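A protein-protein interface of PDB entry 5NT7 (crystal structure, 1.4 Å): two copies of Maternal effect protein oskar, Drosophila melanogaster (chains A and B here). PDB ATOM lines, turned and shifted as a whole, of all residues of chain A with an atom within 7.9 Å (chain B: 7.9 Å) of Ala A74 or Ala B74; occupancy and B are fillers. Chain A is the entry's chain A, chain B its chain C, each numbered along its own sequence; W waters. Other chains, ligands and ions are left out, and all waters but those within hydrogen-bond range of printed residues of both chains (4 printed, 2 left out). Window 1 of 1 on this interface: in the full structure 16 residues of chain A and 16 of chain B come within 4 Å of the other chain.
Of chain B, only Leu B67, Thr B73 and Ala B74 come within 4 Å of Ala A74. Of the printed residues of chain B, Glu A75 touches Val B72 (3.5 Å) and Lys B87 (3.5 Å). Of the printed residues of chain A, Leu B67 touches Thr A63, Leu A67, Ala A74, Cys A76 and Arg A82. Of chain A, only Leu A67 (3.9 Å), Thr A73 (3.2 Å) and Ala A74 (2.9 Å) come within 4 Å of Ala B74. Phe B84 touches none of the printed residues of chain A. The nearest residue of chain B that does not touch Ala A74 is Val B72 (4.2 Å). The nearest residue of chain A that does not touch Ala B74 is Val A72 (4.2 Å).
CD1 of Leu B67 touches CG2 of Thr A63, at 3.7 Å. CG2 of Thr B63 touches CD1 of Leu A67 (3.7 Å). Ala B74 touches Leu A67. CA of Thr A73 touches O of Ala B74, 3.2 Å away. Ala A74 touches Leu B67 (CB to CD1, 3.9 Å). Ala A74 touches Thr B73 (O to CA, 3.2 Å). CA of Glu A75 touches O of Val B72, 3.5 Å away. Glu A75 touches Lys B87 (OE1 to CE, 3.5 Å).
The side-chain hydroxyl (OG1) of Thr A63 lies within hydrogen-bond range of the guanidinium group (NH1) of Arg A82, at 3.0 Å. N of Glu A75 sits at hydrogen-bond distance from O of Ile A83 (2.8 Å). O of Asn B85 lies within hydrogen-bond range of N of Thr B73, 2.9 Å away.
Leu B67 touches its own counterpart, Leu A67. Leu A67 touches Ala B74, and with the chains exchanged Ala A74 touches Leu B67. Val A72 touches Glu B75, and with the chains exchanged Glu A75 touches Val B72. Val A72 touches Cys B76, and with the chains exchanged Cys A76 touches Val B72.
Water W3 lies within hydrogen-bond range of O of Leu A67 (2.6 Å), NE of Arg B82 (3.1 Å) and SG of Cys B76 (3.5 Å). Water W2 lies within hydrogen-bond range of the guanidinium group (NH2) of Arg A82 and the backbone carbonyl oxygen (O) of Leu B67. Water W4 bridges the guanidinium group of Arg B82 (3.2 Å) and the backbone carbonyl oxygen of Leu A67 (3.4 Å).
The side-chain sulfur (SG) of Cys B76 sits close to the backbone carbonyl oxygen (O) of Leu A67 (3.5 Å). The backbone carbonyl oxygen of Leu A67 sits at hydrogen-bond distance from the guanidinium group of Arg B82, 3.2 Å away. The backbone NH of Asn A71 sits at hydrogen-bond distance from the backbone carbonyl oxygen of Cys B76, at 2.8 Å. O of Val A72 lies within hydrogen-bond range of N of Cys B76 (3.0 Å). The backbone carbonyl oxygen (O) of Ala A74 lies within hydrogen-bond range of the backbone NH (N) of Ala B74 (2.9 Å). The side-chain sulfur (SG) of Cys A76 sits close to the backbone carbonyl oxygen (O) of Leu B67, 3.5 Å away. The backbone NH (N) of Asn B71 is in hydrogen-bond range of the backbone carbonyl oxygen (O) of Cys A76. The backbone carbonyl oxygen (O) of Val B72 lies within hydrogen-bond range of the backbone NH (N) of Cys A76 (2.9 Å). The guanidinium group of Arg A82 sits at hydrogen-bond distance from the backbone carbonyl oxygen of Leu B67 (3.2 Å).
Hydrophobic or aromatic side chains of chain B within 4 Å of the printed part of chain A: Leu B67 and Ala B74. Of the 19 printed residues of chain A, 10 touch a printed residue of chain B. Hydrophobic or aromatic side chains of chain A that line the printed part of chain B: Leu A67 and Ala A74. Among the printed residues, 20 pairs touch across the chains.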
ATOM      1  N   LEU A  31      32.302   0.042 -27.723  1.00  0.00           N
ATOM      2  CA  LEU A  31      31.172  -0.722 -28.254  1.00  0.00           C
ATOM      3  C   LEU A  31      30.705  -0.169 -29.599  1.00  0.00           C
ATOM      4  O   LEU A  31      30.392  -0.924 -30.534  1.00  0.00           O
ATOM      5  CB  LEU A  31      30.014  -0.716 -27.253  1.00  0.00           C
ATOM      6  CG  LEU A  31      30.274  -1.386 -25.905  1.00  0.00           C
ATOM      7  CD1 LEU A  31      29.097  -1.203 -24.968  1.00  0.00           C
ATOM      8  CD2 LEU A  31      30.536  -2.846 -26.104  1.00  0.00           C
ATOM      9  N   ILE A  39      30.890  -7.288 -29.181  1.00  0.00           N
ATOM     10  CA  ILE A  39      32.192  -7.564 -28.598  1.00  0.00           C
ATOM     11  C   ILE A  39      32.046  -8.258 -27.231  1.00  0.00           C
ATOM     12  O   ILE A  39      31.134  -7.954 -26.453  1.00  0.00           O
ATOM     13  CB  ILE A  39      32.997  -6.236 -28.518  1.00  0.00           C
ATOM     14  CG1 ILE A  39      34.427  -6.454 -28.057  1.00  0.00           C
ATOM     15  CG2 ILE A  39      32.327  -5.264 -27.610  1.00  0.00           C
ATOM     16  CD1 ILE A  39      35.257  -5.177 -28.062  1.00  0.00           C
ATOM     17  N   THR A  63      29.524  -8.108 -16.442  1.00  0.00           N
ATOM     18  CA  THR A  63      28.250  -7.967 -17.140  1.00  0.00           C
ATOM     19  C   THR A  63      27.326  -6.993 -16.407  1.00  0.00           C
ATOM     20  O   THR A  63      26.710  -6.115 -17.020  1.00  0.00           O
ATOM     21  CB  THR A  63      27.532  -9.323 -17.251  1.00  0.00           C
ATOM     22  OG1 THR A  63      28.248 -10.180 -18.154  1.00  0.00           O
ATOM     23  CG2 THR A  63      26.100  -9.133 -17.757  1.00  0.00           C
ATOM     24  N   LEU A  66      28.601  -3.393 -16.854  1.00  0.00           N
ATOM     25  CA  LEU A  66      28.390  -2.856 -18.200  1.00  0.00           C
ATOM     26  C   LEU A  66      26.928  -2.475 -18.377  1.00  0.00           C
ATOM     27  O   LEU A  66      26.614  -1.483 -19.039  1.00  0.00           O
ATOM     28  CB  LEU A  66      28.811  -3.855 -19.275  1.00  0.00           C
ATOM     29  CG  LEU A  66      30.309  -4.128 -19.369  1.00  0.00           C
ATOM     30  CD1 LEU A  66      30.580  -5.310 -20.278  1.00  0.00           C
ATOM     31  CD2 LEU A  66      31.068  -2.882 -19.860  1.00  0.00           C
ATOM     32  N   LEU A  67      26.043  -3.260 -17.762  1.00  0.00           N
ATOM     33  CA  LEU A  67      24.612  -3.004 -17.871  1.00  0.00           C
ATOM     34  C   LEU A  67      24.107  -1.904 -16.929  1.00  0.00           C
ATOM     35  O   LEU A  67      22.895  -1.680 -16.815  1.00  0.00           O
ATOM     36  CB  LEU A  67      23.800  -4.306 -17.727  1.00  0.00           C
ATOM     37  CG  LEU A  67      23.932  -5.196 -18.961  1.00  0.00           C
ATOM     38  CD1 LEU A  67      23.344  -6.574 -18.699  1.00  0.00           C
ATOM     39  CD2 LEU A  67      23.249  -4.540 -20.160  1.00  0.00           C
ATOM     40  N   ASN A  71      22.437   2.838 -22.399  1.00  0.00           N
ATOM     41  CA  ASN A  71      22.456   2.427 -23.807  1.00  0.00           C
ATOM     42  C   ASN A  71      23.277   1.187 -24.137  1.00  0.00           C
ATOM     43  O   ASN A  71      23.289   0.747 -25.285  1.00  0.00           O
ATOM     44  CB  ASN A  71      22.824   3.583 -24.746  1.00  0.00           C
ATOM     45  CG  ASN A  71      21.795   4.685 -24.729  1.00  0.00           C
ATOM     46  OD1 ASN A  71      20.586   4.428 -24.818  1.00  0.00           O
ATOM     47  ND2 ASN A  71      22.260   5.918 -24.595  1.00  0.00           N
ATOM     48  N   VAL A  72      23.960   0.623 -23.146  1.00  0.00           N
ATOM     49  CA  VAL A  72      24.690  -0.625 -23.367  1.00  0.00           C
ATOM     50  C   VAL A  72      23.739  -1.813 -23.430  1.00  0.00           C
ATOM     51  O   VAL A  72      22.762  -1.887 -22.672  1.00  0.00           O
ATOM     52  CB  VAL A  72      25.791  -0.842 -22.298  1.00  0.00           C
ATOM     53  CG1 VAL A  72      26.429  -2.228 -22.419  1.00  0.00           C
ATOM     54  CG2 VAL A  72      26.862   0.220 -22.473  1.00  0.00           C
ATOM     55  N   THR A  73      24.001  -2.722 -24.370  1.00  0.00           N
ATOM     56  CA  THR A  73      23.191  -3.927 -24.504  1.00  0.00           C
ATOM     57  C   THR A  73      24.071  -5.159 -24.364  1.00  0.00           C
ATOM     58  O   THR A  73      25.299  -5.092 -24.528  1.00  0.00           O
ATOM     59  CB  THR A  73      22.478  -4.011 -25.869  1.00  0.00           C
ATOM     60  OG1 THR A  73      23.440  -4.215 -26.910  1.00  0.00           O
ATOM     61  CG2 THR A  73      21.670  -2.754 -26.149  1.00  0.00           C
ATOM     62  N   ALA A  74      23.426  -6.276 -24.048  1.00  0.00           N
ATOM     63  CA  ALA A  74      24.089  -7.563 -23.971  1.00  0.00           C
ATOM     64  C   ALA A  74      23.183  -8.590 -24.626  1.00  0.00           C
ATOM     65  O   ALA A  74      21.962  -8.450 -24.599  1.00  0.00           O
ATOM     66  CB  ALA A  74      24.357  -7.932 -22.531  1.00  0.00           C
ATOM     67  N   GLU A  75      23.780  -9.606 -25.228  1.00  0.00           N
ATOM     68  CA  GLU A  75      23.026 -10.659 -25.897  1.00  0.00           C
ATOM     69  C   GLU A  75      23.689 -11.992 -25.638  1.00  0.00           C
ATOM     70  O   GLU A  75      24.907 -12.110 -25.702  1.00  0.00           O
ATOM     71  CB  GLU A  75      22.986 -10.397 -27.410  1.00  0.00           C
ATOM     72  CG  GLU A  75      22.414 -11.540 -28.233  1.00  0.00           C
ATOM     73  CD  GLU A  75      22.670 -11.394 -29.726  1.00  0.00           C
ATOM     74  OE1 GLU A  75      22.985 -10.271 -30.181  1.00  0.00           O
ATOM     75  OE2 GLU A  75      22.548 -12.413 -30.440  1.00  0.00           O
ATOM     76  N   CYS A  76      22.890 -13.002 -25.337  1.00  0.00           N
ATOM     77  CA  CYS A  76      23.406 -14.356 -25.366  1.00  0.00           C
ATOM     78  C   CYS A  76      23.231 -14.865 -26.791  1.00  0.00           C
ATOM     79  O   CYS A  76      22.121 -15.193 -27.211  1.00  0.00           O
ATOM     80  CB  CYS A  76      22.663 -15.248 -24.364  1.00  0.00           C
ATOM     81  SG  CYS A  76      23.285 -16.937 -24.312  1.00  0.00           S
ATOM     82  N   SER A  77      24.313 -14.880 -27.560  1.00  0.00           N
ATOM     83  CA  SER A  77      24.211 -15.275 -28.954  1.00  0.00           C
ATOM     84  C   SER A  77      23.952 -16.780 -29.062  1.00  0.00           C
ATOM     85  O   SER A  77      24.217 -17.536 -28.127  1.00  0.00           O
ATOM     86  CB  SER A  77      25.486 -14.898 -29.707  1.00  0.00           C
ATOM     87  OG  SER A  77      26.567 -15.689 -29.259  1.00  0.00           O
ATOM     88  N   LYS A  81      28.354 -17.214 -27.073  1.00  0.00           N
ATOM     89  CA  LYS A  81      29.125 -16.072 -26.607  1.00  0.00           C
ATOM     90  C   LYS A  81      28.210 -14.982 -26.084  1.00  0.00           C
ATOM     91  O   LYS A  81      27.125 -14.751 -26.616  1.00  0.00           O
ATOM     92  CB  LYS A  81      29.982 -15.497 -27.731  1.00  0.00           C
ATOM     93  CG  LYS A  81      30.847 -16.512 -28.442  1.00  0.00           C
ATOM     94  CD  LYS A  81      31.657 -15.839 -29.540  1.00  0.00           C
ATOM     95  CE  LYS A  81      32.860 -15.130 -28.967  1.00  0.00           C
ATOM     96  NZ  LYS A  81      33.768 -16.114 -28.317  1.00  0.00           N
ATOM     97  N   ARG A  82      28.668 -14.297 -25.044  1.00  0.00           N
ATOM     98  CA  ARG A  82      27.944 -13.151 -24.527  1.00  0.00           C
ATOM     99  C   ARG A  82      28.527 -11.911 -25.178  1.00  0.00           C
ATOM    100  O   ARG A  82      29.703 -11.602 -25.002  1.00  0.00           O
ATOM    101  CB  ARG A  82      28.061 -13.078 -23.010  1.00  0.00           C
ATOM    102  CG  ARG A  82      27.214 -11.984 -22.398  1.00  0.00           C
ATOM    103  CD  ARG A  82      27.218 -12.065 -20.888  1.00  0.00           C
ATOM    104  NE  ARG A  82      26.579 -13.303 -20.430  1.00  0.00           N
ATOM    105  CZ  ARG A  82      26.325 -13.583 -19.159  1.00  0.00           C
ATOM    106  NH1 ARG A  82      26.633 -12.717 -18.201  1.00  0.00           N
ATOM    107  NH2 ARG A  82      25.732 -14.730 -18.848  1.00  0.00           N
ATOM    108  N   ILE A  83      27.703 -11.216 -25.951  1.00  0.00           N
ATOM    109  CA  ILE A  83      28.199 -10.099 -26.737  1.00  0.00           C
ATOM    110  C   ILE A  83      27.517  -8.802 -26.363  1.00  0.00           C
ATOM    111  O   ILE A  83      26.313  -8.741 -26.128  1.00  0.00           O
ATOM    112  CB  ILE A  83      28.106 -10.355 -28.259  1.00  0.00           C
ATOM    113  CG1 ILE A  83      26.656 -10.495 -28.715  1.00  0.00           C
ATOM    114  CG2 ILE A  83      28.896 -11.600 -28.643  1.00  0.00           C
ATOM    115  CD1 ILE A  83      26.519 -10.665 -30.223  1.00  0.00           C
ATOM    116  N   PHE A  84      28.318  -7.746 -26.311  1.00  0.00           N
ATOM    117  CA  PHE A  84      27.841  -6.450 -25.869  1.00  0.00           C
ATOM    118  C   PHE A  84      27.824  -5.489 -27.038  1.00  0.00           C
ATOM    119  O   PHE A  84      28.632  -5.604 -27.962  1.00  0.00           O
ATOM    120  CB  PHE A  84      28.726  -5.926 -24.734  1.00  0.00           C
ATOM    121  CG  PHE A  84      28.592  -6.730 -23.478  1.00  0.00           C
ATOM    122  CD1 PHE A  84      27.710  -6.339 -22.481  1.00  0.00           C
ATOM    123  CD2 PHE A  84      29.306  -7.911 -23.316  1.00  0.00           C
ATOM    124  CE1 PHE A  84      27.559  -7.095 -21.333  1.00  0.00           C
ATOM    125  CE2 PHE A  84      29.148  -8.681 -22.162  1.00  0.00           C
ATOM    126  CZ  PHE A  84      28.277  -8.264 -21.171  1.00  0.00           C
ATOM    127  N   ASN A  85      26.888  -4.549 -26.994  1.00  0.00           N
ATOM    128  CA  ASN A  85      26.677  -3.625 -28.086  1.00  0.00           C
ATOM    129  C   ASN A  85      26.015  -2.367 -27.532  1.00  0.00           C
ATOM    130  O   ASN A  85      26.037  -2.134 -26.324  1.00  0.00           O
ATOM    131  CB  ASN A  85      25.847  -4.277 -29.192  1.00  0.00           C
ATOM    132  CG  ASN A  85      26.199  -3.766 -30.573  1.00  0.00           C
ATOM    133  OD1 ASN A  85      26.273  -2.564 -30.798  1.00  0.00           O
ATOM    134  ND2 ASN A  85      26.414  -4.688 -31.514  1.00  0.00           N
ATOM    135  N   LEU A  86      25.413  -1.569 -28.401  1.00  0.00           N
ATOM    136  CA  LEU A  86      24.997  -0.235 -28.008  1.00  0.00           C
ATOM    137  C   LEU A  86      23.730   0.174 -28.727  1.00  0.00           C
ATOM    138  O   LEU A  86      23.569  -0.130 -29.907  1.00  0.00           O
ATOM    139  CB  LEU A  86      26.115   0.747 -28.388  1.00  0.00           C
ATOM    140  CG  LEU A  86      26.044   2.175 -27.875  1.00  0.00           C
ATOM    141  CD1 LEU A  86      26.156   2.167 -26.363  1.00  0.00           C
ATOM    142  CD2 LEU A  86      27.143   3.013 -28.492  1.00  0.00           C
ATOM    143  N   LYS A  87      22.836   0.867 -28.019  1.00  0.00           N
ATOM    144  CA  LYS A  87      21.694   1.537 -28.640  1.00  0.00           C
ATOM    145  C   LYS A  87      22.083   2.973 -28.974  1.00  0.00           C
ATOM    146  O   LYS A  87      22.897   3.587 -28.272  1.00  0.00           O
ATOM    147  CB  LYS A  87      20.500   1.577 -27.692  1.00  0.00           C
ATOM    148  CG  LYS A  87      19.932   0.222 -27.320  1.00  0.00           C
ATOM    149  CD  LYS A  87      19.339  -0.486 -28.522  1.00  0.00           C
ATOM    150  CE  LYS A  87      18.505  -1.672 -28.076  1.00  0.00           C
ATOM    151  NZ  LYS A  87      17.946  -2.428 -29.222  1.00  0.00           N
ATOM    152  N   LEU B  31       9.378 -13.240 -22.736  1.00  0.00           N
ATOM    153  CA  LEU B  31      10.039 -12.101 -23.367  1.00  0.00           C
ATOM    154  C   LEU B  31       9.437 -11.837 -24.747  1.00  0.00           C
ATOM    155  O   LEU B  31       9.210 -10.683 -25.136  1.00  0.00           O
ATOM    156  CB  LEU B  31      11.537 -12.367 -23.484  1.00  0.00           C
ATOM    157  CG  LEU B  31      12.346 -12.531 -22.196  1.00  0.00           C
ATOM    158  CD1 LEU B  31      13.794 -12.885 -22.495  1.00  0.00           C
ATOM    159  CD2 LEU B  31      12.298 -11.277 -21.389  1.00  0.00           C
ATOM    160  N   ILE B  39      10.970  -6.012 -20.921  1.00  0.00           N
ATOM    161  CA  ILE B  39      10.388  -6.319 -19.626  1.00  0.00           C
ATOM    162  C   ILE B  39      11.484  -6.377 -18.565  1.00  0.00           C
ATOM    163  O   ILE B  39      12.597  -6.840 -18.832  1.00  0.00           O
ATOM    164  CB  ILE B  39       9.591  -7.644 -19.721  1.00  0.00           C
ATOM    165  CG1 ILE B  39       8.980  -8.037 -18.390  1.00  0.00           C
ATOM    166  CG2 ILE B  39      10.466  -8.752 -20.203  1.00  0.00           C
ATOM    167  CD1 ILE B  39       8.067  -9.253 -18.504  1.00  0.00           C
ATOM    168  N   THR B  63      20.242 -11.282 -13.786  1.00  0.00           N
ATOM    169  CA  THR B  63      20.715 -10.793 -15.075  1.00  0.00           C
ATOM    170  C   THR B  63      21.674 -11.809 -15.692  1.00  0.00           C
ATOM    171  O   THR B  63      21.568 -12.152 -16.874  1.00  0.00           O
ATOM    172  CB  THR B  63      21.444  -9.444 -14.932  1.00  0.00           C
ATOM    173  OG1 THR B  63      20.508  -8.425 -14.562  1.00  0.00           O
ATOM    174  CG2 THR B  63      22.125  -9.052 -16.246  1.00  0.00           C
ATOM    175  N   LEU B  66      19.730 -14.895 -16.863  1.00  0.00           N
ATOM    176  CA  LEU B  66      18.952 -14.660 -18.079  1.00  0.00           C
ATOM    177  C   LEU B  66      19.851 -14.628 -19.308  1.00  0.00           C
ATOM    178  O   LEU B  66      19.458 -15.091 -20.378  1.00  0.00           O
ATOM    179  CB  LEU B  66      18.162 -13.362 -17.976  1.00  0.00           C
ATOM    180  CG  LEU B  66      17.047 -13.406 -16.939  1.00  0.00           C
ATOM    181  CD1 LEU B  66      16.457 -12.030 -16.743  1.00  0.00           C
ATOM    182  CD2 LEU B  66      15.969 -14.418 -17.374  1.00  0.00           C
ATOM    183  N   LEU B  67      21.060 -14.085 -19.139  1.00  0.00           N
ATOM    184  CA  LEU B  67      22.017 -13.984 -20.239  1.00  0.00           C
ATOM    185  C   LEU B  67      22.795 -15.287 -20.502  1.00  0.00           C
ATOM    186  O   LEU B  67      23.731 -15.302 -21.299  1.00  0.00           O
ATOM    187  CB  LEU B  67      22.963 -12.793 -20.027  1.00  0.00           C
ATOM    188  CG  LEU B  67      22.247 -11.449 -20.152  1.00  0.00           C
ATOM    189  CD1 LEU B  67      23.136 -10.302 -19.657  1.00  0.00           C
ATOM    190  CD2 LEU B  67      21.827 -11.196 -21.588  1.00  0.00           C
ATOM    191  N   ASN B  71      19.591 -16.279 -27.166  1.00  0.00           N
ATOM    192  CA  ASN B  71      18.756 -15.259 -27.798  1.00  0.00           C
ATOM    193  C   ASN B  71      18.190 -14.190 -26.871  1.00  0.00           C
ATOM    194  O   ASN B  71      17.533 -13.250 -27.328  1.00  0.00           O
ATOM    195  CB  ASN B  71      17.655 -15.881 -28.656  1.00  0.00           C
ATOM    196  CG  ASN B  71      18.217 -16.697 -29.789  1.00  0.00           C
ATOM    197  OD1 ASN B  71      19.109 -16.239 -30.507  1.00  0.00           O
ATOM    198  ND2 ASN B  71      17.735 -17.921 -29.935  1.00  0.00           N
ATOM    199  N   VAL B  72      18.441 -14.331 -25.575  1.00  0.00           N
ATOM    200  CA  VAL B  72      17.980 -13.332 -24.620  1.00  0.00           C
ATOM    201  C   VAL B  72      18.882 -12.108 -24.671  1.00  0.00           C
ATOM    202  O   VAL B  72      20.111 -12.233 -24.747  1.00  0.00           O
ATOM    203  CB  VAL B  72      17.872 -13.900 -23.185  1.00  0.00           C
ATOM    204  CG1 VAL B  72      17.614 -12.790 -22.168  1.00  0.00           C
ATOM    205  CG2 VAL B  72      16.753 -14.930 -23.123  1.00  0.00           C
ATOM    206  N   THR B  73      18.269 -10.931 -24.649  1.00  0.00           N
ATOM    207  CA  THR B  73      19.025  -9.684 -24.637  1.00  0.00           C
ATOM    208  C   THR B  73      18.696  -8.863 -23.405  1.00  0.00           C
ATOM    209  O   THR B  73      17.642  -9.032 -22.787  1.00  0.00           O
ATOM    210  CB  THR B  73      18.732  -8.833 -25.877  1.00  0.00           C
ATOM    211  OG1 THR B  73      17.389  -8.331 -25.817  1.00  0.00           O
ATOM    212  CG2 THR B  73      18.917  -9.643 -27.135  1.00  0.00           C
ATOM    213  N   ALA B  74      19.610  -7.964 -23.054  1.00  0.00           N
ATOM    214  CA  ALA B  74      19.397  -7.032 -21.961  1.00  0.00           C
ATOM    215  C   ALA B  74      19.854  -5.660 -22.423  1.00  0.00           C
ATOM    216  O   ALA B  74      20.762  -5.557 -23.249  1.00  0.00           O
ATOM    217  CB  ALA B  74      20.187  -7.463 -20.736  1.00  0.00           C
ATOM    218  N   GLU B  75      19.227  -4.614 -21.896  1.00  0.00           N
ATOM    219  CA  GLU B  75      19.572  -3.245 -22.258  1.00  0.00           C
ATOM    220  C   GLU B  75      19.481  -2.364 -21.035  1.00  0.00           C
ATOM    221  O   GLU B  75      18.548  -2.474 -20.255  1.00  0.00           O
ATOM    222  CB  GLU B  75      18.607  -2.706 -23.328  1.00  0.00           C
ATOM    223  CG  GLU B  75      18.655  -1.190 -23.520  1.00  0.00           C
ATOM    224  CD  GLU B  75      17.509  -0.664 -24.375  1.00  0.00           C
ATOM    225  OE1 GLU B  75      16.871  -1.474 -25.078  1.00  0.00           O
ATOM    226  OE2 GLU B  75      17.249   0.561 -24.340  1.00  0.00           O
ATOM    227  N   CYS B  76      20.453  -1.478 -20.864  1.00  0.00           N
ATOM    228  CA  CYS B  76      20.310  -0.416 -19.885  1.00  0.00           C
ATOM    229  C   CYS B  76      19.625   0.746 -20.591  1.00  0.00           C
ATOM    230  O   CYS B  76      20.259   1.476 -21.361  1.00  0.00           O
ATOM    231  CB  CYS B  76      21.677  -0.005 -19.340  1.00  0.00           C
ATOM    232  SG  CYS B  76      21.606   1.269 -18.080  1.00  0.00           S
ATOM    233  N   SER B  77      18.327   0.908 -20.362  1.00  0.00           N
ATOM    234  CA  SER B  77      17.590   1.967 -21.041  1.00  0.00           C
ATOM    235  C   SER B  77      18.058   3.333 -20.550  1.00  0.00           C
ATOM    236  O   SER B  77      18.644   3.452 -19.471  1.00  0.00           O
ATOM    237  CB  SER B  77      16.084   1.807 -20.830  1.00  0.00           C
ATOM    238  OG  SER B  77      15.727   2.170 -19.512  1.00  0.00           O
ATOM    239  N   LYS B  81      16.132   1.884 -16.348  1.00  0.00           N
ATOM    240  CA  LYS B  81      15.646   0.520 -16.168  1.00  0.00           C
ATOM    241  C   LYS B  81      16.441  -0.488 -16.985  1.00  0.00           C
ATOM    242  O   LYS B  81      16.841  -0.216 -18.120  1.00  0.00           O
ATOM    243  CB  LYS B  81      14.170   0.407 -16.543  1.00  0.00           C
ATOM    244  CG  LYS B  81      13.229   1.187 -15.637  1.00  0.00           C
ATOM    245  CD  LYS B  81      11.781   0.923 -16.017  1.00  0.00           C
ATOM    246  CE  LYS B  81      10.821   1.722 -15.142  1.00  0.00           C
ATOM    247  NZ  LYS B  81       9.400   1.436 -15.486  1.00  0.00           N
ATOM    248  N   ARG B  82      16.650  -1.663 -16.403  1.00  0.00           N
ATOM    249  CA  ARG B  82      17.266  -2.769 -17.115  1.00  0.00           C
ATOM    250  C   ARG B  82      16.152  -3.599 -17.737  1.00  0.00           C
ATOM    251  O   ARG B  82      15.307  -4.146 -17.030  1.00  0.00           O
ATOM    252  CB  ARG B  82      18.132  -3.602 -16.172  1.00  0.00           C
ATOM    253  CG  ARG B  82      18.935  -4.683 -16.870  1.00  0.00           C
ATOM    254  CD  ARG B  82      19.918  -5.339 -15.923  1.00  0.00           C
ATOM    255  NE  ARG B  82      20.913  -4.369 -15.457  1.00  0.00           N
ATOM    256  CZ  ARG B  82      21.965  -4.668 -14.706  1.00  0.00           C
ATOM    257  NH1 ARG B  82      22.204  -5.916 -14.334  1.00  0.00           N
ATOM    258  NH2 ARG B  82      22.804  -3.702 -14.343  1.00  0.00           N
ATOM    259  N   ILE B  83      16.164  -3.659 -19.064  1.00  0.00           N
ATOM    260  CA  ILE B  83      15.069  -4.215 -19.861  1.00  0.00           C
ATOM    261  C   ILE B  83      15.549  -5.428 -20.638  1.00  0.00           C
ATOM    262  O   ILE B  83      16.583  -5.374 -21.301  1.00  0.00           O
ATOM    263  CB  ILE B  83      14.580  -3.140 -20.852  1.00  0.00           C
ATOM    264  CG1 ILE B  83      14.007  -1.959 -20.076  1.00  0.00           C
ATOM    265  CG2 ILE B  83      13.537  -3.683 -21.794  1.00  0.00           C
ATOM    266  CD1 ILE B  83      12.898  -2.376 -19.159  1.00  0.00           C
ATOM    267  N   PHE B  84      14.795  -6.523 -20.557  1.00  0.00           N
ATOM    268  CA  PHE B  84      15.154  -7.750 -21.261  1.00  0.00           C
ATOM    269  C   PHE B  84      14.236  -8.000 -22.448  1.00  0.00           C
ATOM    270  O   PHE B  84      13.070  -7.602 -22.445  1.00  0.00           O
ATOM    271  CB  PHE B  84      15.151  -8.947 -20.300  1.00  0.00           C
ATOM    272  CG  PHE B  84      16.196  -8.842 -19.232  1.00  0.00           C
ATOM    273  CD1 PHE B  84      17.398  -9.519 -19.362  1.00  0.00           C
ATOM    274  CD2 PHE B  84      15.992  -8.030 -18.123  1.00  0.00           C
ATOM    275  CE1 PHE B  84      18.377  -9.406 -18.386  1.00  0.00           C
ATOM    276  CE2 PHE B  84      16.975  -7.901 -17.147  1.00  0.00           C
ATOM    277  CZ  PHE B  84      18.162  -8.597 -17.278  1.00  0.00           C
ATOM    278  N   ASN B  85      14.783  -8.654 -23.465  1.00  0.00           N
ATOM    279  CA  ASN B  85      14.068  -8.874 -24.708  1.00  0.00           C
ATOM    280  C   ASN B  85      14.684 -10.078 -25.411  1.00  0.00           C
ATOM    281  O   ASN B  85      15.408 -10.847 -24.789  1.00  0.00           O
ATOM    282  CB  ASN B  85      14.115  -7.611 -25.583  1.00  0.00           C
ATOM    283  CG  ASN B  85      12.886  -7.450 -26.464  1.00  0.00           C
ATOM    284  OD1 ASN B  85      12.447  -8.391 -27.125  1.00  0.00           O
ATOM    285  ND2 ASN B  85      12.330  -6.243 -26.483  1.00  0.00           N
ATOM    286  N   LEU B  86      14.425 -10.215 -26.704  1.00  0.00           N
ATOM    287  CA  LEU B  86      14.718 -11.452 -27.403  1.00  0.00           C
ATOM    288  C   LEU B  86      15.170 -11.200 -28.832  1.00  0.00           C
ATOM    289  O   LEU B  86      14.669 -10.297 -29.490  1.00  0.00           O
ATOM    290  CB  LEU B  86      13.439 -12.302 -27.434  1.00  0.00           C
ATOM    291  CG  LEU B  86      13.540 -13.759 -27.868  1.00  0.00           C
ATOM    292  CD1 LEU B  86      14.429 -14.531 -26.905  1.00  0.00           C
ATOM    293  CD2 LEU B  86      12.161 -14.393 -27.950  1.00  0.00           C
ATOM    294  N   LYS B  87      16.111 -12.007 -29.311  1.00  0.00           N
ATOM    295  CA  LYS B  87      16.456 -12.035 -30.726  1.00  0.00           C
ATOM    296  C   LYS B  87      15.673 -13.159 -31.386  1.00  0.00           C
ATOM    297  O   LYS B  87      15.392 -14.176 -30.748  1.00  0.00           O
ATOM    298  CB  LYS B  87      17.945 -12.317 -30.916  1.00  0.00           C
ATOM    299  CG  LYS B  87      18.870 -11.248 -30.379  1.00  0.00           C
ATOM    300  CD  LYS B  87      18.693  -9.939 -31.119  1.00  0.00           C
ATOM    301  CE  LYS B  87      19.777  -8.942 -30.727  1.00  0.00           C
ATOM    302  NZ  LYS B  87      19.483  -7.567 -31.216  1.00  0.00           N
HETATM  303  O   HOH W   1      20.997 -14.457 -31.037  1.00  0.00           O
HETATM  304  O   HOH W   2      26.495 -16.965 -20.747  1.00  0.00           O
HETATM  305  O   HOH W   3      20.351  -1.487 -16.313  1.00  0.00           O
HETATM  306  O   HOH W   4      21.250  -0.983 -13.949  1.00  0.00           O
